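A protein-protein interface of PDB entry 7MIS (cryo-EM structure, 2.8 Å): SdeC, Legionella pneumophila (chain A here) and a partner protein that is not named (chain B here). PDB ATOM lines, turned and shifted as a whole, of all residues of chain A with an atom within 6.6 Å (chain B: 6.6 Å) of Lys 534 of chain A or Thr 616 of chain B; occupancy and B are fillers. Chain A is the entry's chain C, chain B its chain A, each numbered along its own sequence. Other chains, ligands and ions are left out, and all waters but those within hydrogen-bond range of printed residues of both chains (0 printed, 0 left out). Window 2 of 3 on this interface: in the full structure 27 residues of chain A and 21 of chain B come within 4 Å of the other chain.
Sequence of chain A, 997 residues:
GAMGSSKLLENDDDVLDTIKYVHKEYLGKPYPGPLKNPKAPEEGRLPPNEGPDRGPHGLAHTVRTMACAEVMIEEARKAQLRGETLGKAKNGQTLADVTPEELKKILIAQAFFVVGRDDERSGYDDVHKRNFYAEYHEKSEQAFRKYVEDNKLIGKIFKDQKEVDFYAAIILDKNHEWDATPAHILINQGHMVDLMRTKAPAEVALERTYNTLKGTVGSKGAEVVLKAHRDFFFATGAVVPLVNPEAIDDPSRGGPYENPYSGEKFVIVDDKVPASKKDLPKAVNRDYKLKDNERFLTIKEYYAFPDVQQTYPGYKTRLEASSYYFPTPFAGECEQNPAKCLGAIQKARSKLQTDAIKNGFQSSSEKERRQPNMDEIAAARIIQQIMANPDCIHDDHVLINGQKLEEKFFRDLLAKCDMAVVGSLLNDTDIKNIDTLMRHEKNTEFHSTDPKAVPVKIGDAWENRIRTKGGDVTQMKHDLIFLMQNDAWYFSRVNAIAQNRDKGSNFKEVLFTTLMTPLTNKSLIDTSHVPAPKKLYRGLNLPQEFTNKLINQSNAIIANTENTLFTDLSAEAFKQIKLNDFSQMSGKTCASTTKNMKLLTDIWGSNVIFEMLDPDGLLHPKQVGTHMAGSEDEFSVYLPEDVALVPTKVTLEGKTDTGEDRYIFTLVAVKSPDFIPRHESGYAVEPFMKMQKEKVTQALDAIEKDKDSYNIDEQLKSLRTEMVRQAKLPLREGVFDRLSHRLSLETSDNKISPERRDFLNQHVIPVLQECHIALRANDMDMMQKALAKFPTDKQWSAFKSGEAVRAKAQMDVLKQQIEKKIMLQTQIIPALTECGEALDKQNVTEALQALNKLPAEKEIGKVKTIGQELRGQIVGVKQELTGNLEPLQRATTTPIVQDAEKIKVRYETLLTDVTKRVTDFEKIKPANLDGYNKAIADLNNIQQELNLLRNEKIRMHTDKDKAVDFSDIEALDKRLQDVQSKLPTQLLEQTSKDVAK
OG1 of Thr 616 of chain B is in hydrogen-bond range of O of Ala 532 of chain A, 3.3 Å away.
The side-chain hydroxyl (OG1) of Thr 616 of chain B sits at hydrogen-bond distance from the guanidinium group (NH2) of Arg 639 of chain B, at 3.3 Å.
The backbone NH of Tyr 637 of chain B sits at hydrogen-bond distance from the side-chain carboxylate of Asp 617 of chain B (2.8 Å).
O of Lys 534 of chain A is in hydrogen-bond range of N of Asp 614 of chain A, at 2.7 Å.
Pro 531 of chain A touches Thr 616 of chain B (CB to OG1, 3.7 Å).
Pro 531 of chain A touches Asp 617 of chain B (CG to OD1, 2.9 Å).
Arg 639 of chain B touches Pro 533 of chain A (NH2 to CA, 3.9 Å).
Thr 616 of chain B touches Lys 534 of chain A (CG2 to NZ, 3.4 Å).
Printed residues of chain B within 4 Å of Pro 531 of chain A: Thr 616 (3.7 Å) and Asp 617 (2.9 Å).
Of the printed residues of chain B, Ala 532 of chain A touches Thr 616 (3.3 Å).
Of chain B, only Thr 616 (3.4 Å) comes within 4 Å of Lys 534 of chain A.
Of the printed residues of chain A, Asp 617 of chain B touches Pro 531 (2.9 Å).
Printed residues of chain A within 4 Å of Arg 639 of chain B: Pro 533 (3.9 Å).
The nearest printed residue of chain B that does not touch Pro 531 of chain A is Tyr 637 of chain B (4.4 Å).
Of the 9 printed residues of chain B, 3 touch a printed residue of chain A.
Of the 14 printed residues of chain A, 4 touch a printed residue of chain B.
Hydrophobic or aromatic side chains of chain A that line the printed part of chain B: Pro 531.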
ATOM      1  N   PRO A 531     -19.252  24.397 -14.273  1.00  0.00           N
ATOM      2  CA  PRO A 531     -20.367  24.643 -13.351  1.00  0.00           C
ATOM      3  C   PRO A 531     -21.229  25.809 -13.813  1.00  0.00           C
ATOM      4  O   PRO A 531     -20.754  26.751 -14.449  1.00  0.00           O
ATOM      5  CB  PRO A 531     -19.675  24.950 -12.016  1.00  0.00           C
ATOM      6  CG  PRO A 531     -18.238  25.157 -12.335  1.00  0.00           C
ATOM      7  CD  PRO A 531     -17.946  24.440 -13.597  1.00  0.00           C
ATOM      8  N   ALA A 532     -22.514  25.732 -13.475  1.00  0.00           N
ATOM      9  CA  ALA A 532     -23.503  26.672 -13.985  1.00  0.00           C
ATOM     10  C   ALA A 532     -23.593  27.892 -13.079  1.00  0.00           C
ATOM     11  O   ALA A 532     -23.832  27.734 -11.874  1.00  0.00           O
ATOM     12  CB  ALA A 532     -24.863  26.006 -14.079  1.00  0.00           C
ATOM     13  N   PRO A 533     -23.418  29.108 -13.593  1.00  0.00           N
ATOM     14  CA  PRO A 533     -23.639  30.290 -12.757  1.00  0.00           C
ATOM     15  C   PRO A 533     -25.109  30.453 -12.404  1.00  0.00           C
ATOM     16  O   PRO A 533     -25.999  29.987 -13.118  1.00  0.00           O
ATOM     17  CB  PRO A 533     -23.144  31.446 -13.632  1.00  0.00           C
ATOM     18  CG  PRO A 533     -23.237  30.943 -15.015  1.00  0.00           C
ATOM     19  CD  PRO A 533     -22.980  29.473 -14.951  1.00  0.00           C
ATOM     20  N   LYS A 534     -25.354  31.125 -11.280  1.00  0.00           N
ATOM     21  CA  LYS A 534     -26.712  31.340 -10.800  1.00  0.00           C
ATOM     22  C   LYS A 534     -27.320  32.652 -11.277  1.00  0.00           C
ATOM     23  O   LYS A 534     -28.548  32.768 -11.309  1.00  0.00           O
ATOM     24  CB  LYS A 534     -26.737  31.311  -9.271  1.00  0.00           C
ATOM     25  CG  LYS A 534     -26.293  29.994  -8.676  1.00  0.00           C
ATOM     26  CD  LYS A 534     -26.464  29.977  -7.168  1.00  0.00           C
ATOM     27  CE  LYS A 534     -25.696  31.104  -6.489  1.00  0.00           C
ATOM     28  NZ  LYS A 534     -24.282  31.202  -6.952  1.00  0.00           N
ATOM     29  N   LYS A 535     -26.500  33.634 -11.632  1.00  0.00           N
ATOM     30  CA  LYS A 535     -26.967  34.907 -12.163  1.00  0.00           C
ATOM     31  C   LYS A 535     -26.554  35.014 -13.622  1.00  0.00           C
ATOM     32  O   LYS A 535     -25.409  34.713 -13.968  1.00  0.00           O
ATOM     33  CB  LYS A 535     -26.386  36.086 -11.380  1.00  0.00           C
ATOM     34  CG  LYS A 535     -27.030  36.330 -10.037  1.00  0.00           C
ATOM     35  CD  LYS A 535     -26.527  37.625  -9.421  1.00  0.00           C
ATOM     36  CE  LYS A 535     -26.994  37.785  -7.982  1.00  0.00           C
ATOM     37  NZ  LYS A 535     -26.480  36.704  -7.096  1.00  0.00           N
ATOM     38  N   LEU A 536     -27.481  35.446 -14.470  1.00  0.00           N
ATOM     39  CA  LEU A 536     -27.167  35.666 -15.874  1.00  0.00           C
ATOM     40  C   LEU A 536     -27.763  36.993 -16.310  1.00  0.00           C
ATOM     41  O   LEU A 536     -28.697  37.504 -15.698  1.00  0.00           O
ATOM     42  CB  LEU A 536     -27.683  34.524 -16.756  1.00  0.00           C
ATOM     43  CG  LEU A 536     -26.895  33.218 -16.644  1.00  0.00           C
ATOM     44  CD1 LEU A 536     -27.595  32.113 -17.406  1.00  0.00           C
ATOM     45  CD2 LEU A 536     -25.474  33.393 -17.146  1.00  0.00           C
ATOM     46  N   MET A 612     -31.379  37.483 -14.729  1.00  0.00           N
ATOM     47  CA  MET A 612     -32.072  36.239 -14.434  1.00  0.00           C
ATOM     48  C   MET A 612     -31.394  35.568 -13.248  1.00  0.00           C
ATOM     49  O   MET A 612     -30.201  35.243 -13.311  1.00  0.00           O
ATOM     50  CB  MET A 612     -32.057  35.315 -15.651  1.00  0.00           C
ATOM     51  CG  MET A 612     -32.497  35.975 -16.950  1.00  0.00           C
ATOM     52  SD  MET A 612     -31.865  35.115 -18.399  1.00  0.00           S
ATOM     53  CE  MET A 612     -33.030  35.651 -19.645  1.00  0.00           C
ATOM     54  N   LEU A 613     -32.155  35.366 -12.177  1.00  0.00           N
ATOM     55  CA  LEU A 613     -31.680  34.698 -10.975  1.00  0.00           C
ATOM     56  C   LEU A 613     -32.135  33.246 -11.000  1.00  0.00           C
ATOM     57  O   LEU A 613     -33.315  32.964 -11.227  1.00  0.00           O
ATOM     58  CB  LEU A 613     -32.208  35.393  -9.721  1.00  0.00           C
ATOM     59  CG  LEU A 613     -32.046  36.912  -9.667  1.00  0.00           C
ATOM     60  CD1 LEU A 613     -32.410  37.431  -8.288  1.00  0.00           C
ATOM     61  CD2 LEU A 613     -30.632  37.320 -10.030  1.00  0.00           C
ATOM     62  N   ASP A 614     -31.197  32.333 -10.769  1.00  0.00           N
ATOM     63  CA  ASP A 614     -31.460  30.896 -10.826  1.00  0.00           C
ATOM     64  C   ASP A 614     -30.873  30.219  -9.594  1.00  0.00           C
ATOM     65  O   ASP A 614     -29.994  29.359  -9.695  1.00  0.00           O
ATOM     66  CB  ASP A 614     -30.878  30.310 -12.109  1.00  0.00           C
ATOM     67  CG  ASP A 614     -31.493  28.983 -12.475  1.00  0.00           C
ATOM     68  OD1 ASP A 614     -32.722  28.832 -12.316  1.00  0.00           O
ATOM     69  OD2 ASP A 614     -30.749  28.089 -12.927  1.00  0.00           O
ATOM     70  N   PRO A 615     -31.344  30.585  -8.401  1.00  0.00           N
ATOM     71  CA  PRO A 615     -30.797  29.966  -7.184  1.00  0.00           C
ATOM     72  C   PRO A 615     -30.992  28.462  -7.132  1.00  0.00           C
ATOM     73  O   PRO A 615     -30.135  27.755  -6.589  1.00  0.00           O
ATOM     74  CB  PRO A 615     -31.557  30.677  -6.057  1.00  0.00           C
ATOM     75  CG  PRO A 615     -32.791  31.206  -6.693  1.00  0.00           C
ATOM     76  CD  PRO A 615     -32.428  31.536  -8.102  1.00  0.00           C
ATOM     77  N   ASP A 616     -32.093  27.950  -7.679  1.00  0.00           N
ATOM     78  CA  ASP A 616     -32.388  26.525  -7.637  1.00  0.00           C
ATOM     79  C   ASP A 616     -31.735  25.738  -8.764  1.00  0.00           C
ATOM     80  O   ASP A 616     -31.703  24.506  -8.695  1.00  0.00           O
ATOM     81  CB  ASP A 616     -33.902  26.306  -7.683  1.00  0.00           C
ATOM     82  CG  ASP A 616     -34.617  26.938  -6.505  1.00  0.00           C
ATOM     83  OD1 ASP A 616     -34.128  26.796  -5.365  1.00  0.00           O
ATOM     84  OD2 ASP A 616     -35.669  27.577  -6.719  1.00  0.00           O
ATOM     85  N   GLY A 617     -31.217  26.406  -9.793  1.00  0.00           N
ATOM     86  CA  GLY A 617     -30.570  25.713 -10.890  1.00  0.00           C
ATOM     87  C   GLY A 617     -31.554  25.125 -11.880  1.00  0.00           C
ATOM     88  O   GLY A 617     -31.468  23.944 -12.222  1.00  0.00           O
ATOM     89  N   LEU A 619     -32.204  26.378 -15.052  1.00  0.00           N
ATOM     90  CA  LEU A 619     -31.986  26.857 -16.412  1.00  0.00           C
ATOM     91  C   LEU A 619     -30.945  26.069 -17.190  1.00  0.00           C
ATOM     92  O   LEU A 619     -31.009  26.045 -18.420  1.00  0.00           O
ATOM     93  CB  LEU A 619     -31.571  28.333 -16.391  1.00  0.00           C
ATOM     94  CG  LEU A 619     -32.629  29.304 -15.865  1.00  0.00           C
ATOM     95  CD1 LEU A 619     -32.107  30.730 -15.876  1.00  0.00           C
ATOM     96  CD2 LEU A 619     -33.906  29.201 -16.674  1.00  0.00           C
ATOM     97  N   PRO A 621     -27.557  26.547 -17.839  1.00  0.00           N
ATOM     98  CA  PRO A 621     -26.734  27.280 -18.804  1.00  0.00           C
ATOM     99  C   PRO A 621     -25.535  26.455 -19.240  1.00  0.00           C
ATOM    100  O   PRO A 621     -24.964  25.685 -18.466  1.00  0.00           O
ATOM    101  CB  PRO A 621     -26.297  28.531 -18.033  1.00  0.00           C
ATOM    102  CG  PRO A 621     -27.114  28.554 -16.792  1.00  0.00           C
ATOM    103  CD  PRO A 621     -27.488  27.151 -16.501  1.00  0.00           C
ATOM    104  N   GLU B 596     -23.276  25.749   3.287  1.00  0.00           N
ATOM    105  CA  GLU B 596     -23.504  26.991   2.555  1.00  0.00           C
ATOM    106  C   GLU B 596     -23.761  28.157   3.503  1.00  0.00           C
ATOM    107  O   GLU B 596     -23.133  29.217   3.390  1.00  0.00           O
ATOM    108  CB  GLU B 596     -24.679  26.818   1.591  1.00  0.00           C
ATOM    109  CG  GLU B 596     -24.618  27.728   0.376  1.00  0.00           C
ATOM    110  CD  GLU B 596     -25.806  27.553  -0.551  1.00  0.00           C
ATOM    111  OE1 GLU B 596     -26.952  27.516  -0.054  1.00  0.00           O
ATOM    112  OE2 GLU B 596     -25.595  27.454  -1.778  1.00  0.00           O
ATOM    113  N   GLU B 614     -18.390  34.940  -4.768  1.00  0.00           N
ATOM    114  CA  GLU B 614     -19.439  34.078  -5.293  1.00  0.00           C
ATOM    115  C   GLU B 614     -18.813  32.953  -6.103  1.00  0.00           C
ATOM    116  O   GLU B 614     -17.914  33.195  -6.913  1.00  0.00           O
ATOM    117  CB  GLU B 614     -20.410  34.873  -6.168  1.00  0.00           C
ATOM    118  CG  GLU B 614     -21.222  35.918  -5.421  1.00  0.00           C
ATOM    119  CD  GLU B 614     -22.196  35.305  -4.437  1.00  0.00           C
ATOM    120  OE1 GLU B 614     -22.692  34.192  -4.707  1.00  0.00           O
ATOM    121  OE2 GLU B 614     -22.473  35.940  -3.398  1.00  0.00           O
ATOM    122  N   PHE B 615     -19.286  31.730  -5.882  1.00  0.00           N
ATOM    123  CA  PHE B 615     -18.819  30.592  -6.657  1.00  0.00           C
ATOM    124  C   PHE B 615     -19.872  29.497  -6.603  1.00  0.00           C
ATOM    125  O   PHE B 615     -20.494  29.279  -5.561  1.00  0.00           O
ATOM    126  CB  PHE B 615     -17.472  30.071  -6.138  1.00  0.00           C
ATOM    127  CG  PHE B 615     -17.536  29.469  -4.763  1.00  0.00           C
ATOM    128  CD1 PHE B 615     -17.786  28.121  -4.595  1.00  0.00           C
ATOM    129  CD2 PHE B 615     -17.332  30.251  -3.639  1.00  0.00           C
ATOM    130  CE1 PHE B 615     -17.840  27.566  -3.334  1.00  0.00           C
ATOM    131  CE2 PHE B 615     -17.385  29.699  -2.376  1.00  0.00           C
ATOM    132  CZ  PHE B 615     -17.639  28.355  -2.225  1.00  0.00           C
ATOM    133  N   THR B 616     -20.072  28.822  -7.733  1.00  0.00           N
ATOM    134  CA  THR B 616     -20.971  27.680  -7.817  1.00  0.00           C
ATOM    135  C   THR B 616     -20.229  26.352  -7.831  1.00  0.00           C
ATOM    136  O   THR B 616     -20.858  25.309  -8.027  1.00  0.00           O
ATOM    137  CB  THR B 616     -21.848  27.781  -9.070  1.00  0.00           C
ATOM    138  OG1 THR B 616     -21.017  27.893 -10.231  1.00  0.00           O
ATOM    139  CG2 THR B 616     -22.763  28.986  -8.986  1.00  0.00           C
ATOM    140  N   ASP B 617     -18.916  26.365  -7.632  1.00  0.00           N
ATOM    141  CA  ASP B 617     -18.139  25.139  -7.671  1.00  0.00           C
ATOM    142  C   ASP B 617     -18.479  24.256  -6.475  1.00  0.00           C
ATOM    143  O   ASP B 617     -18.924  24.727  -5.426  1.00  0.00           O
ATOM    144  CB  ASP B 617     -16.645  25.456  -7.666  1.00  0.00           C
ATOM    145  CG  ASP B 617     -16.205  26.214  -8.898  1.00  0.00           C
ATOM    146  OD1 ASP B 617     -16.839  26.068  -9.957  1.00  0.00           O
ATOM    147  OD2 ASP B 617     -15.214  26.958  -8.808  1.00  0.00           O
ATOM    148  N   LYS B 618     -18.261  22.956  -6.642  1.00  0.00           N
ATOM    149  CA  LYS B 618     -18.488  21.994  -5.574  1.00  0.00           C
ATOM    150  C   LYS B 618     -17.187  21.778  -4.812  1.00  0.00           C
ATOM    151  O   LYS B 618     -16.195  21.316  -5.384  1.00  0.00           O
ATOM    152  CB  LYS B 618     -19.006  20.669  -6.131  1.00  0.00           C
ATOM    153  CG  LYS B 618     -19.278  19.625  -5.059  1.00  0.00           C
ATOM    154  CD  LYS B 618     -19.909  18.372  -5.638  1.00  0.00           C
ATOM    155  CE  LYS B 618     -20.140  17.321  -4.564  1.00  0.00           C
ATOM    156  NZ  LYS B 618     -20.957  17.839  -3.429  1.00  0.00           N
ATOM    157  N   LEU B 625     -11.561  24.435  -3.123  1.00  0.00           N
ATOM    158  CA  LEU B 625     -11.738  24.632  -4.554  1.00  0.00           C
ATOM    159  C   LEU B 625     -10.557  24.012  -5.289  1.00  0.00           C
ATOM    160  O   LEU B 625      -9.407  24.404  -5.067  1.00  0.00           O
ATOM    161  CB  LEU B 625     -11.857  26.118  -4.879  1.00  0.00           C
ATOM    162  CG  LEU B 625     -13.082  26.831  -4.308  1.00  0.00           C
ATOM    163  CD1 LEU B 625     -12.822  28.319  -4.187  1.00  0.00           C
ATOM    164  CD2 LEU B 625     -14.299  26.568  -5.169  1.00  0.00           C
ATOM    165  N   TYR B 637     -13.458  27.959 -10.695  1.00  0.00           N
ATOM    166  CA  TYR B 637     -13.201  27.854 -12.125  1.00  0.00           C
ATOM    167  C   TYR B 637     -13.980  28.919 -12.885  1.00  0.00           C
ATOM    168  O   TYR B 637     -15.184  29.090 -12.683  1.00  0.00           O
ATOM    169  CB  TYR B 637     -13.583  26.466 -12.630  1.00  0.00           C
ATOM    170  CG  TYR B 637     -13.305  26.280 -14.101  1.00  0.00           C
ATOM    171  CD1 TYR B 637     -12.025  26.010 -14.553  1.00  0.00           C
ATOM    172  CD2 TYR B 637     -14.318  26.392 -15.036  1.00  0.00           C
ATOM    173  CE1 TYR B 637     -11.764  25.846 -15.893  1.00  0.00           C
ATOM    174  CE2 TYR B 637     -14.067  26.231 -16.381  1.00  0.00           C
ATOM    175  CZ  TYR B 637     -12.787  25.958 -16.804  1.00  0.00           C
ATOM    176  OH  TYR B 637     -12.532  25.797 -18.145  1.00  0.00           O
ATOM    177  N   ARG B 639     -13.866  31.943 -12.442  1.00  0.00           N
ATOM    178  CA  ARG B 639     -14.154  33.052 -11.547  1.00  0.00           C
ATOM    179  C   ARG B 639     -12.879  33.837 -11.278  1.00  0.00           C
ATOM    180  O   ARG B 639     -11.780  33.443 -11.676  1.00  0.00           O
ATOM    181  CB  ARG B 639     -14.751  32.551 -10.227  1.00  0.00           C
ATOM    182  CG  ARG B 639     -15.948  31.635 -10.387  1.00  0.00           C
ATOM    183  CD  ARG B 639     -17.136  32.371 -10.968  1.00  0.00           C
ATOM    184  NE  ARG B 639     -18.355  31.571 -10.894  1.00  0.00           N
ATOM    185  CZ  ARG B 639     -19.529  32.008 -10.458  1.00  0.00           C
ATOM    186  NH1 ARG B 639     -19.698  33.251 -10.036  1.00  0.00           N
ATOM    187  NH2 ARG B 639     -20.565  31.175 -10.447  1.00  0.00           N
